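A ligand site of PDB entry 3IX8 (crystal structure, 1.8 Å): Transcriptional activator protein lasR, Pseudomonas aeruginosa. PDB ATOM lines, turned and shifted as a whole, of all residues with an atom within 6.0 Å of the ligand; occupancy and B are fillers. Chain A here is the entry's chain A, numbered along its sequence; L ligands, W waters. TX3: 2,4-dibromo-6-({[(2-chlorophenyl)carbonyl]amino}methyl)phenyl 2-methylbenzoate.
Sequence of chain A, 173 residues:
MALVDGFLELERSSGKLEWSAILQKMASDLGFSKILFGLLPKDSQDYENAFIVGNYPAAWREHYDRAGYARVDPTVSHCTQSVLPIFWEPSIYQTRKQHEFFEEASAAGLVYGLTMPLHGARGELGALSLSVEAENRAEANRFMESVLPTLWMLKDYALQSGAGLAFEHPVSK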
ATOM      1  N   LEU A  36      -9.999  25.561  21.069  1.00  0.00           N
ATOM      2  CA  LEU A  36     -11.372  26.006  21.104  1.00  0.00           C
ATOM      3  C   LEU A  36     -12.143  24.995  21.933  1.00  0.00           C
ATOM      4  O   LEU A  36     -12.088  23.784  21.660  1.00  0.00           O
ATOM      5  CB  LEU A  36     -11.977  26.146  19.697  1.00  0.00           C
ATOM      6  CG  LEU A  36     -13.469  26.528  19.644  1.00  0.00           C
ATOM      7  CD1 LEU A  36     -13.760  27.463  18.479  1.00  0.00           C
ATOM      8  CD2 LEU A  36     -14.379  25.297  19.597  1.00  0.00           C
ATOM      9  N   PHE A  37     -12.847  25.513  22.941  1.00  0.00           N
ATOM     10  CA  PHE A  37     -13.803  24.749  23.721  1.00  0.00           C
ATOM     11  C   PHE A  37     -15.154  25.320  23.351  1.00  0.00           C
ATOM     12  O   PHE A  37     -15.420  26.510  23.562  1.00  0.00           O
ATOM     13  CB  PHE A  37     -13.517  24.936  25.223  1.00  0.00           C
ATOM     14  CG  PHE A  37     -14.534  24.298  26.148  1.00  0.00           C
ATOM     15  CD1 PHE A  37     -14.307  23.033  26.695  1.00  0.00           C
ATOM     16  CD2 PHE A  37     -15.707  24.962  26.490  1.00  0.00           C
ATOM     17  CE1 PHE A  37     -15.227  22.450  27.564  1.00  0.00           C
ATOM     18  CE2 PHE A  37     -16.646  24.388  27.338  1.00  0.00           C
ATOM     19  CZ  PHE A  37     -16.404  23.138  27.878  1.00  0.00           C
ATOM     20  N   GLY A  38     -16.018  24.476  22.788  1.00  0.00           N
ATOM     21  CA  GLY A  38     -17.361  24.919  22.434  1.00  0.00           C
ATOM     22  C   GLY A  38     -18.427  24.047  23.056  1.00  0.00           C
ATOM     23  O   GLY A  38     -18.260  22.831  23.164  1.00  0.00           O
ATOM     24  N   LEU A  39     -19.521  24.655  23.492  1.00  0.00           N
ATOM     25  CA  LEU A  39     -20.559  23.931  24.193  1.00  0.00           C
ATOM     26  C   LEU A  39     -21.937  24.480  23.873  1.00  0.00           C
ATOM     27  O   LEU A  39     -22.138  25.685  23.803  1.00  0.00           O
ATOM     28  CB  LEU A  39     -20.313  23.961  25.714  1.00  0.00           C
ATOM     29  CG  LEU A  39     -20.853  22.806  26.578  1.00  0.00           C
ATOM     30  CD1 LEU A  39     -20.233  21.465  26.176  1.00  0.00           C
ATOM     31  CD2 LEU A  39     -20.580  23.064  28.060  1.00  0.00           C
ATOM     32  N   LEU A  40     -22.881  23.563  23.663  1.00  0.00           N
ATOM     33  CA  LEU A  40     -24.291  23.860  23.441  1.00  0.00           C
ATOM     34  C   LEU A  40     -25.126  23.128  24.485  1.00  0.00           C
ATOM     35  O   LEU A  40     -24.760  22.042  24.925  1.00  0.00           O
ATOM     36  CB  LEU A  40     -24.717  23.406  22.039  1.00  0.00           C
ATOM     37  CG  LEU A  40     -24.381  24.330  20.861  1.00  0.00           C
ATOM     38  CD1 LEU A  40     -24.669  23.641  19.540  1.00  0.00           C
ATOM     39  CD2 LEU A  40     -25.139  25.653  20.924  1.00  0.00           C
ATOM     40  N   TYR A  47     -25.419  26.559  16.702  1.00  0.00           N
ATOM     41  CA  TYR A  47     -23.962  26.650  16.722  1.00  0.00           C
ATOM     42  C   TYR A  47     -23.427  28.071  16.730  1.00  0.00           C
ATOM     43  O   TYR A  47     -22.434  28.364  17.394  1.00  0.00           O
ATOM     44  CB  TYR A  47     -23.355  25.874  15.536  1.00  0.00           C
ATOM     45  CG  TYR A  47     -23.495  24.382  15.686  1.00  0.00           C
ATOM     46  CD1 TYR A  47     -22.615  23.656  16.483  1.00  0.00           C
ATOM     47  CD2 TYR A  47     -24.528  23.684  15.040  1.00  0.00           C
ATOM     48  CE1 TYR A  47     -22.735  22.286  16.626  1.00  0.00           C
ATOM     49  CE2 TYR A  47     -24.662  22.298  15.189  1.00  0.00           C
ATOM     50  CZ  TYR A  47     -23.750  21.617  15.981  1.00  0.00           C
ATOM     51  OH  TYR A  47     -23.861  20.241  16.147  1.00  0.00           O
ATOM     52  N   GLU A  48     -24.092  28.950  15.976  1.00  0.00           N
ATOM     53  CA  GLU A  48     -23.715  30.361  15.895  1.00  0.00           C
ATOM     54  C   GLU A  48     -23.852  31.079  17.240  1.00  0.00           C
ATOM     55  O   GLU A  48     -23.307  32.173  17.419  1.00  0.00           O
ATOM     56  CB  GLU A  48     -24.515  31.074  14.814  1.00  0.00           C
ATOM     57  CG  GLU A  48     -24.102  30.715  13.393  1.00  0.00           C
ATOM     58  CD  GLU A  48     -24.848  31.518  12.333  1.00  0.00           C
ATOM     59  OE1 GLU A  48     -25.283  32.655  12.646  1.00  0.00           O
ATOM     60  OE2 GLU A  48     -24.995  31.023  11.194  1.00  0.00           O
ATOM     61  N   ALA A  50     -23.219  29.207  20.258  1.00  0.00           N
ATOM     62  CA  ALA A  50     -22.579  28.313  21.217  1.00  0.00           C
ATOM     63  C   ALA A  50     -21.768  29.109  22.237  1.00  0.00           C
ATOM     64  O   ALA A  50     -21.357  30.245  21.994  1.00  0.00           O
ATOM     65  CB  ALA A  50     -21.685  27.322  20.502  1.00  0.00           C
ATOM     66  N   PHE A  51     -21.551  28.493  23.397  1.00  0.00           N
ATOM     67  CA  PHE A  51     -20.566  28.999  24.354  1.00  0.00           C
ATOM     68  C   PHE A  51     -19.214  28.597  23.785  1.00  0.00           C
ATOM     69  O   PHE A  51     -18.917  27.406  23.666  1.00  0.00           O
ATOM     70  CB  PHE A  51     -20.819  28.363  25.722  1.00  0.00           C
ATOM     71  CG  PHE A  51     -19.779  28.680  26.773  1.00  0.00           C
ATOM     72  CD1 PHE A  51     -19.840  29.864  27.504  1.00  0.00           C
ATOM     73  CD2 PHE A  51     -18.760  27.772  27.070  1.00  0.00           C
ATOM     74  CE1 PHE A  51     -18.877  30.160  28.493  1.00  0.00           C
ATOM     75  CE2 PHE A  51     -17.781  28.050  28.053  1.00  0.00           C
ATOM     76  CZ  PHE A  51     -17.860  29.246  28.771  1.00  0.00           C
ATOM     77  N   ILE A  52     -18.404  29.599  23.405  1.00  0.00           N
ATOM     78  CA  ILE A  52     -17.069  29.374  22.838  1.00  0.00           C
ATOM     79  C   ILE A  52     -15.978  30.013  23.685  1.00  0.00           C
ATOM     80  O   ILE A  52     -16.093  31.190  24.076  1.00  0.00           O
ATOM     81  CB  ILE A  52     -16.969  29.937  21.387  1.00  0.00           C
ATOM     82  CG1 ILE A  52     -18.026  29.308  20.462  1.00  0.00           C
ATOM     83  CG2 ILE A  52     -15.548  29.765  20.818  1.00  0.00           C
ATOM     84  CD1 ILE A  52     -17.748  27.880  20.059  1.00  0.00           C
ATOM     85  N   TYR A  56      -8.514  30.664  19.150  1.00  0.00           N
ATOM     86  CA  TYR A  56      -8.612  30.690  17.686  1.00  0.00           C
ATOM     87  C   TYR A  56      -8.646  32.146  17.246  1.00  0.00           C
ATOM     88  O   TYR A  56      -9.214  32.996  17.947  1.00  0.00           O
ATOM     89  CB  TYR A  56      -9.899  30.007  17.191  1.00  0.00           C
ATOM     90  CG  TYR A  56      -9.834  28.510  17.045  1.00  0.00           C
ATOM     91  CD1 TYR A  56      -8.885  27.734  17.705  1.00  0.00           C
ATOM     92  CD2 TYR A  56     -10.779  27.833  16.229  1.00  0.00           C
ATOM     93  CE1 TYR A  56      -8.842  26.353  17.567  1.00  0.00           C
ATOM     94  CE2 TYR A  56     -10.747  26.455  16.092  1.00  0.00           C
ATOM     95  CZ  TYR A  56      -9.787  25.719  16.750  1.00  0.00           C
ATOM     96  OH  TYR A  56      -9.754  24.343  16.622  1.00  0.00           O
ATOM     97  N   TRP A  60     -11.100  34.328  12.079  1.00  0.00           N
ATOM     98  CA  TRP A  60     -11.494  32.972  11.706  1.00  0.00           C
ATOM     99  C   TRP A  60     -12.833  32.573  12.344  1.00  0.00           C
ATOM    100  O   TRP A  60     -13.726  32.060  11.644  1.00  0.00           O
ATOM    101  CB  TRP A  60     -10.417  31.928  12.028  1.00  0.00           C
ATOM    102  CG  TRP A  60     -10.880  30.507  11.805  1.00  0.00           C
ATOM    103  CD1 TRP A  60     -10.937  29.506  12.723  1.00  0.00           C
ATOM    104  CD2 TRP A  60     -11.354  29.944  10.564  1.00  0.00           C
ATOM    105  NE1 TRP A  60     -11.398  28.336  12.132  1.00  0.00           N
ATOM    106  CE2 TRP A  60     -11.674  28.596  10.821  1.00  0.00           C
ATOM    107  CE3 TRP A  60     -11.535  30.454   9.266  1.00  0.00           C
ATOM    108  CZ2 TRP A  60     -12.171  27.736   9.817  1.00  0.00           C
ATOM    109  CZ3 TRP A  60     -12.030  29.599   8.281  1.00  0.00           C
ATOM    110  CH2 TRP A  60     -12.339  28.257   8.567  1.00  0.00           C
ATOM    111  N   ARG A  61     -12.960  32.800  13.646  1.00  0.00           N
ATOM    112  CA  ARG A  61     -14.207  32.475  14.349  1.00  0.00           C
ATOM    113  C   ARG A  61     -15.374  33.208  13.687  1.00  0.00           C
ATOM    114  O   ARG A  61     -16.457  32.638  13.509  1.00  0.00           O
ATOM    115  CB  ARG A  61     -14.107  32.786  15.860  1.00  0.00           C
ATOM    116  CG  ARG A  61     -13.219  31.769  16.628  1.00  0.00           C
ATOM    117  CD  ARG A  61     -12.988  32.103  18.111  1.00  0.00           C
ATOM    118  NE  ARG A  61     -12.684  33.509  18.330  1.00  0.00           N
ATOM    119  CZ  ARG A  61     -11.748  33.985  19.153  1.00  0.00           C
ATOM    120  NH1 ARG A  61     -10.961  33.180  19.866  1.00  0.00           N
ATOM    121  NH2 ARG A  61     -11.602  35.296  19.255  1.00  0.00           N
ATOM    122  N   TYR A  64     -16.168  31.628  10.200  1.00  0.00           N
ATOM    123  CA  TYR A  64     -16.832  30.348  10.431  1.00  0.00           C
ATOM    124  C   TYR A  64     -18.329  30.544  10.674  1.00  0.00           C
ATOM    125  O   TYR A  64     -19.159  29.836  10.090  1.00  0.00           O
ATOM    126  CB  TYR A  64     -16.162  29.649  11.623  1.00  0.00           C
ATOM    127  CG  TYR A  64     -16.603  28.230  11.899  1.00  0.00           C
ATOM    128  CD1 TYR A  64     -15.751  27.156  11.641  1.00  0.00           C
ATOM    129  CD2 TYR A  64     -17.839  27.950  12.484  1.00  0.00           C
ATOM    130  CE1 TYR A  64     -16.126  25.835  11.904  1.00  0.00           C
ATOM    131  CE2 TYR A  64     -18.233  26.636  12.757  1.00  0.00           C
ATOM    132  CZ  TYR A  64     -17.366  25.579  12.461  1.00  0.00           C
ATOM    133  OH  TYR A  64     -17.736  24.279  12.728  1.00  0.00           O
ATOM    134  N   ASP A  65     -18.686  31.497  11.527  1.00  0.00           N
ATOM    135  CA  ASP A  65     -20.094  31.803  11.815  1.00  0.00           C
ATOM    136  C   ASP A  65     -20.824  32.343  10.581  1.00  0.00           C
ATOM    137  O   ASP A  65     -21.966  31.950  10.303  1.00  0.00           O
ATOM    138  CB  ASP A  65     -20.226  32.786  12.977  1.00  0.00           C
ATOM    139  CG  ASP A  65     -20.124  32.122  14.337  1.00  0.00           C
ATOM    140  OD1 ASP A  65     -19.857  30.898  14.398  1.00  0.00           O
ATOM    141  OD2 ASP A  65     -20.329  32.820  15.359  1.00  0.00           O
ATOM    142  N   ALA A  70     -20.462  25.293  10.511  1.00  0.00           N
ATOM    143  CA  ALA A  70     -20.866  24.224  11.413  1.00  0.00           C
ATOM    144  C   ALA A  70     -21.570  23.077  10.666  1.00  0.00           C
ATOM    145  O   ALA A  70     -21.492  21.914  11.079  1.00  0.00           O
ATOM    146  CB  ALA A  70     -21.740  24.762  12.554  1.00  0.00           C
ATOM    147  N   ASP A  73     -18.187  21.530   8.474  1.00  0.00           N
ATOM    148  CA  ASP A  73     -17.088  21.061   9.304  1.00  0.00           C
ATOM    149  C   ASP A  73     -17.246  19.581   9.650  1.00  0.00           C
ATOM    150  O   ASP A  73     -18.186  19.207  10.344  1.00  0.00           O
ATOM    151  CB  ASP A  73     -17.077  21.916  10.587  1.00  0.00           C
ATOM    152  CG  ASP A  73     -15.928  21.605  11.512  1.00  0.00           C
ATOM    153  OD1 ASP A  73     -15.262  20.566  11.351  1.00  0.00           O
ATOM    154  OD2 ASP A  73     -15.721  22.419  12.447  1.00  0.00           O
ATOM    155  N   THR A  75     -15.645  17.790  11.681  1.00  0.00           N
ATOM    156  CA  THR A  75     -15.507  17.473  13.113  1.00  0.00           C
ATOM    157  C   THR A  75     -16.844  17.610  13.843  1.00  0.00           C
ATOM    158  O   THR A  75     -17.143  16.834  14.766  1.00  0.00           O
ATOM    159  CB  THR A  75     -14.397  18.310  13.816  1.00  0.00           C
ATOM    160  OG1 THR A  75     -14.803  19.683  13.911  1.00  0.00           O
ATOM    161  CG2 THR A  75     -13.107  18.235  13.040  1.00  0.00           C
ATOM    162  N   VAL A  76     -17.642  18.574  13.419  1.00  0.00           N
ATOM    163  CA  VAL A  76     -18.962  18.817  14.022  1.00  0.00           C
ATOM    164  C   VAL A  76     -19.869  17.600  13.814  1.00  0.00           C
ATOM    165  O   VAL A  76     -20.478  17.103  14.760  1.00  0.00           O
ATOM    166  CB  VAL A  76     -19.596  20.107  13.468  1.00  0.00           C
ATOM    167  CG1 VAL A  76     -21.054  20.253  13.922  1.00  0.00           C
ATOM    168  CG2 VAL A  76     -18.782  21.326  13.913  1.00  0.00           C
ATOM    169  N   CYS A  79     -18.732  14.745  15.966  1.00  0.00           N
ATOM    170  CA  CYS A  79     -19.135  14.902  17.372  1.00  0.00           C
ATOM    171  C   CYS A  79     -20.549  14.450  17.676  1.00  0.00           C
ATOM    172  O   CYS A  79     -20.832  13.981  18.767  1.00  0.00           O
ATOM    173  CB  CYS A  79     -18.933  16.351  17.816  1.00  0.00           C
ATOM    174  SG  CYS A  79     -17.208  16.768  17.990  1.00  0.00           S
ATOM    175  N   TRP A  88      -7.264  15.563  12.668  1.00  0.00           N
ATOM    176  CA  TRP A  88      -7.404  16.440  11.509  1.00  0.00           C
ATOM    177  C   TRP A  88      -6.481  15.934  10.407  1.00  0.00           C
ATOM    178  O   TRP A  88      -5.280  16.195  10.417  1.00  0.00           O
ATOM    179  CB  TRP A  88      -7.048  17.888  11.837  1.00  0.00           C
ATOM    180  CG  TRP A  88      -7.791  18.493  13.021  1.00  0.00           C
ATOM    181  CD1 TRP A  88      -8.914  18.008  13.626  1.00  0.00           C
ATOM    182  CD2 TRP A  88      -7.462  19.711  13.691  1.00  0.00           C
ATOM    183  NE1 TRP A  88      -9.298  18.852  14.660  1.00  0.00           N
ATOM    184  CE2 TRP A  88      -8.424  19.902  14.722  1.00  0.00           C
ATOM    185  CE3 TRP A  88      -6.447  20.665  13.530  1.00  0.00           C
ATOM    186  CZ2 TRP A  88      -8.390  21.013  15.571  1.00  0.00           C
ATOM    187  CZ3 TRP A  88      -6.415  21.768  14.382  1.00  0.00           C
ATOM    188  CH2 TRP A  88      -7.396  21.925  15.393  1.00  0.00           C
ATOM    189  N   ILE A  92     -10.514  13.540   6.121  1.00  0.00           N
ATOM    190  CA  ILE A  92     -11.811  13.876   6.726  1.00  0.00           C
ATOM    191  C   ILE A  92     -12.571  14.950   5.932  1.00  0.00           C
ATOM    192  O   ILE A  92     -13.770  15.146   6.142  1.00  0.00           O
ATOM    193  CB  ILE A  92     -11.734  14.258   8.238  1.00  0.00           C
ATOM    194  CG1 ILE A  92     -11.022  15.603   8.455  1.00  0.00           C
ATOM    195  CG2 ILE A  92     -11.111  13.130   9.059  1.00  0.00           C
ATOM    196  CD1 ILE A  92     -11.193  16.187   9.895  1.00  0.00           C
ATOM    197  N   TYR A  93     -11.861  15.641   5.035  1.00  0.00           N
ATOM    198  CA  TYR A  93     -12.439  16.661   4.180  1.00  0.00           C
ATOM    199  C   TYR A  93     -12.761  16.046   2.829  1.00  0.00           C
ATOM    200  O   TYR A  93     -11.874  15.886   1.972  1.00  0.00           O
ATOM    201  CB  TYR A  93     -11.462  17.834   4.030  1.00  0.00           C
ATOM    202  CG  TYR A  93     -10.972  18.377   5.359  1.00  0.00           C
ATOM    203  CD1 TYR A  93     -11.720  19.292   6.085  1.00  0.00           C
ATOM    204  CD2 TYR A  93      -9.750  17.947   5.896  1.00  0.00           C
ATOM    205  CE1 TYR A  93     -11.263  19.791   7.315  1.00  0.00           C
ATOM    206  CE2 TYR A  93      -9.286  18.434   7.128  1.00  0.00           C
ATOM    207  CZ  TYR A  93     -10.042  19.355   7.833  1.00  0.00           C
ATOM    208  OH  TYR A  93      -9.591  19.830   9.048  1.00  0.00           O
ATOM    209  N   PHE A 101     -13.389  24.531   2.995  1.00  0.00           N
ATOM    210  CA  PHE A 101     -13.255  24.730   4.453  1.00  0.00           C
ATOM    211  C   PHE A 101     -11.818  24.456   4.906  1.00  0.00           C
ATOM    212  O   PHE A 101     -11.199  25.267   5.613  1.00  0.00           O
ATOM    213  CB  PHE A 101     -14.258  23.821   5.175  1.00  0.00           C
ATOM    214  CG  PHE A 101     -14.121  23.829   6.679  1.00  0.00           C
ATOM    215  CD1 PHE A 101     -14.650  24.874   7.413  1.00  0.00           C
ATOM    216  CD2 PHE A 101     -13.461  22.804   7.341  1.00  0.00           C
ATOM    217  CE1 PHE A 101     -14.508  24.901   8.806  1.00  0.00           C
ATOM    218  CE2 PHE A 101     -13.311  22.825   8.724  1.00  0.00           C
ATOM    219  CZ  PHE A 101     -13.850  23.872   9.459  1.00  0.00           C
ATOM    220  N   ALA A 105      -9.409  26.998   6.856  1.00  0.00           N
ATOM    221  CA  ALA A 105      -8.940  26.646   8.201  1.00  0.00           C
ATOM    222  C   ALA A 105      -7.417  26.550   8.261  1.00  0.00           C
ATOM    223  O   ALA A 105      -6.804  26.973   9.239  1.00  0.00           O
ATOM    224  CB  ALA A 105      -9.580  25.341   8.679  1.00  0.00           C
ATOM    225  N   LEU A 110      -4.922  26.088  11.221  1.00  0.00           N
ATOM    226  CA  LEU A 110      -5.496  24.837  11.719  1.00  0.00           C
ATOM    227  C   LEU A 110      -5.216  23.704  10.747  1.00  0.00           C
ATOM    228  O   LEU A 110      -6.074  23.332   9.940  1.00  0.00           O
ATOM    229  CB  LEU A 110      -6.997  24.981  11.999  1.00  0.00           C
ATOM    230  CG  LEU A 110      -7.372  26.145  12.927  1.00  0.00           C
ATOM    231  CD1 LEU A 110      -8.875  26.359  12.946  1.00  0.00           C
ATOM    232  CD2 LEU A 110      -6.863  25.909  14.328  1.00  0.00           C
ATOM    233  N   THR A 115      -9.904  16.858  17.494  1.00  0.00           N
ATOM    234  CA  THR A 115     -11.056  17.314  18.220  1.00  0.00           C
ATOM    235  C   THR A 115     -11.612  16.176  19.091  1.00  0.00           C
ATOM    236  O   THR A 115     -11.833  15.056  18.613  1.00  0.00           O
ATOM    237  CB  THR A 115     -12.145  17.825  17.261  1.00  0.00           C
ATOM    238  OG1 THR A 115     -11.625  18.943  16.504  1.00  0.00           O
ATOM    239  CG2 THR A 115     -13.391  18.239  18.018  1.00  0.00           C
ATOM    240  N   LEU A 125     -23.681  19.380  24.430  1.00  0.00           N
ATOM    241  CA  LEU A 125     -22.962  18.882  23.258  1.00  0.00           C
ATOM    242  C   LEU A 125     -21.868  19.864  22.905  1.00  0.00           C
ATOM    243  O   LEU A 125     -22.120  21.069  22.797  1.00  0.00           O
ATOM    244  CB  LEU A 125     -23.915  18.703  22.066  1.00  0.00           C
ATOM    245  CG  LEU A 125     -23.351  18.453  20.665  1.00  0.00           C
ATOM    246  CD1 LEU A 125     -22.792  17.032  20.541  1.00  0.00           C
ATOM    247  CD2 LEU A 125     -24.403  18.740  19.571  1.00  0.00           C
ATOM    248  N   GLY A 126     -20.663  19.368  22.710  1.00  0.00           N
ATOM    249  CA  GLY A 126     -19.548  20.267  22.484  1.00  0.00           C
ATOM    250  C   GLY A 126     -18.330  19.622  21.862  1.00  0.00           C
ATOM    251  O   GLY A 126     -18.384  18.472  21.422  1.00  0.00           O
ATOM    252  N   ALA A 127     -17.231  20.378  21.857  1.00  0.00           N
ATOM    253  CA  ALA A 127     -15.963  19.928  21.309  1.00  0.00           C
ATOM    254  C   ALA A 127     -14.829  20.618  22.044  1.00  0.00           C
ATOM    255  O   ALA A 127     -14.949  21.773  22.463  1.00  0.00           O
ATOM    256  CB  ALA A 127     -15.883  20.249  19.827  1.00  0.00           C
ATOM    257  N   SER A 129     -11.203  21.295  20.669  1.00  0.00           N
ATOM    258  CA  SER A 129     -10.278  21.161  19.550  1.00  0.00           C
ATOM    259  C   SER A 129      -8.942  21.753  19.932  1.00  0.00           C
ATOM    260  O   SER A 129      -8.898  22.741  20.671  1.00  0.00           O
ATOM    261  CB  SER A 129     -10.827  21.847  18.311  1.00  0.00           C
ATOM    262  OG  SER A 129     -12.082  21.293  17.943  1.00  0.00           O
HETATM  263  C1  TX3 L   1     -17.003  25.004  16.191  1.00  0.00           C
HETATM  264  C2  TX3 L   1     -17.532  26.380  16.126  1.00  0.00           C
HETATM  265  C3  TX3 L   1     -16.679  27.389  15.668  1.00  0.00           C
HETATM  266  C4  TX3 L   1     -15.364  27.083  15.272  1.00  0.00           C
HETATM  267  C5  TX3 L   1     -14.845  25.792  15.323  1.00  0.00           C
HETATM  268  C6  TX3 L   1     -15.609  24.727  15.780  1.00  0.00           C
HETATM  269  C7  TX3 L   1     -15.079  23.316  15.835  1.00  0.00           C
HETATM  270  N8  TX3 L   1     -14.219  23.049  14.688  1.00  0.00           N
HETATM  271  C9  TX3 L   1     -12.897  23.057  14.815  1.00  0.00           C
HETATM  272  O10 TX3 L   1     -12.352  23.372  15.873  1.00  0.00           O
HETATM  273  C11 TX3 L   1     -12.032  22.686  13.647  1.00  0.00           C
HETATM  274  C12 TX3 L   1     -11.486  21.419  13.521  1.00  0.00           C
HETATM  275  C13 TX3 L   1     -10.682  21.093  12.417  1.00  0.00           C
HETATM  276  C14 TX3 L   1     -10.423  22.041  11.426  1.00  0.00           C
HETATM  277  C15 TX3 L   1     -10.951  23.338  11.489  1.00  0.00           C
HETATM  278  C16 TX3 L   1     -11.758  23.691  12.575  1.00  0.00           C
HETATM  279 CL17 TX3 L   1     -12.477  25.335  12.696  1.00  0.00          CL
HETATM  280 BR18 TX3 L   1     -19.349  26.699  16.640  1.00  0.00          BR
HETATM  281 BR19 TX3 L   1     -14.227  28.440  14.638  1.00  0.00          BR
HETATM  282  O20 TX3 L   1     -17.778  23.979  16.627  1.00  0.00           O
HETATM  283  C21 TX3 L   1     -18.136  23.825  18.007  1.00  0.00           C
HETATM  284  O22 TX3 L   1     -17.777  24.670  18.817  1.00  0.00           O
HETATM  285  C23 TX3 L   1     -18.937  22.613  18.343  1.00  0.00           C
HETATM  286  C24 TX3 L   1     -18.629  21.388  17.752  1.00  0.00           C
HETATM  287  C25 TX3 L   1     -19.399  20.260  18.072  1.00  0.00           C
HETATM  288  C26 TX3 L   1     -20.459  20.348  18.973  1.00  0.00           C
HETATM  289  C27 TX3 L   1     -20.803  21.555  19.583  1.00  0.00           C
HETATM  290  C28 TX3 L   1     -20.069  22.702  19.292  1.00  0.00           C
HETATM  291  C29 TX3 L   1     -20.424  24.031  19.939  1.00  0.00           C
HETATM  292  O   HOH W   1     -17.246  30.693  15.327  1.00  0.00           O
HETATM  293  O   HOH W   2     -21.942  18.488  16.814  1.00  0.00           O
HETATM  294  O   HOH W   3     -16.234  19.849  16.229  1.00  0.00           O
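The backbone carbonyl oxygen (O) of Leu 125 is in hydrogen-bond range of the backbone NH (N) of Leu 40 (2.7 Å).
O of Phe 51 sits at hydrogen-bond distance from N of Leu 39 (2.8 Å).
The backbone carbonyl oxygen of Ala 127 sits at hydrogen-bond distance from the backbone NH of Gly 38, 2.9 Å away.
O of Ala 105 sits at hydrogen-bond distance from N of Leu 110 (2.9 Å).
The side-chain hydroxyl (OH) of Tyr 64 is in hydrogen-bond range of the side-chain carboxylate (OD2) of Asp 73, at 2.8 Å.
OD1 of Asp 73 sits at hydrogen-bond distance from OG1 of Thr 75 (2.7 Å).
NE1 of Trp 88 lies within hydrogen-bond range of OG1 of Thr 115 (3.0 Å).
The backbone NH of Ser 129 lies within hydrogen-bond range of the backbone carbonyl oxygen of Leu 36 (2.8 Å).
The side-chain carboxylate (OD2) of Asp 73 lies within hydrogen-bond range of a nitrogen (N8) of the ligand.
The side-chain hydroxyl of Ser 129 sits at hydrogen-bond distance from an oxygen (O10) of the ligand (2.9 Å).
The side-chain hydroxyl of Tyr 56 is in hydrogen-bond range of an oxygen (O10) of the ligand, 2.9 Å away.
Water W2 lies within hydrogen-bond range of OH of Tyr 47 (2.7 Å) and O of Val 76 (2.9 Å).
Water W3 lies within hydrogen-bond range of OG1 of Thr 75 (2.7 Å), N of Val 76 (3.4 Å) and SG of Cys 79 (3.7 Å).
Water W1 lies within hydrogen-bond range of the backbone carbonyl oxygen of Arg 61 and the side-chain carboxylate of Asp 65.
Leu 36 touches the ligand (CD2 to O22, 3.5 Å).
Gly 38 touches the ligand (CA to O22, 3.6 Å).
Leu 39 touches the ligand.
O of Tyr 47 touches BR18 of the ligand, at 3.6 Å.
Ala 50 touches the ligand.
CD1 of Ile 52 touches O22 of the ligand (3.4 Å).
NE1 of Trp 60 touches CL17 of the ligand, at 3.2 Å.
CE2 of Tyr 64 touches C3 of the ligand, at 3.4 Å.
OG1 of Thr 75 touches N8 of the ligand, at 3.5 Å.
Val 76 touches the ligand.
Cys 79 touches the ligand.
CE2 of Trp 88 touches C13 of the ligand (3.4 Å).
Tyr 93 touches the ligand (OH to C14, 3.4 Å).
CZ of Phe 101 touches C15 of the ligand, at 3.6 Å.
Ala 105 touches the ligand.
CD1 of Leu 110 touches CL17 of the ligand (3.8 Å).
Thr 115 touches the ligand (OG1 to C12, 3.9 Å).
Leu 125 touches the ligand.
Gly 126 touches the ligand.
Ala 127 touches the ligand (CB to C24, 3.6 Å).
Within 4 Å of the ligand: Leu 36, Gly 38, Leu 39, Tyr 47, Ala 50, Ile 52, Tyr 56, Trp 60, Tyr 64, Asp 73, Thr 75, Val 76, Cys 79, Trp 88, Tyr 93, Phe 101, Ala 105, Leu 110, Thr 115, Leu 125, Gly 126, Ala 127 and Ser 129.
The nearest printed residue that does not touch the ligand is Arg 61 (4.01 Å).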
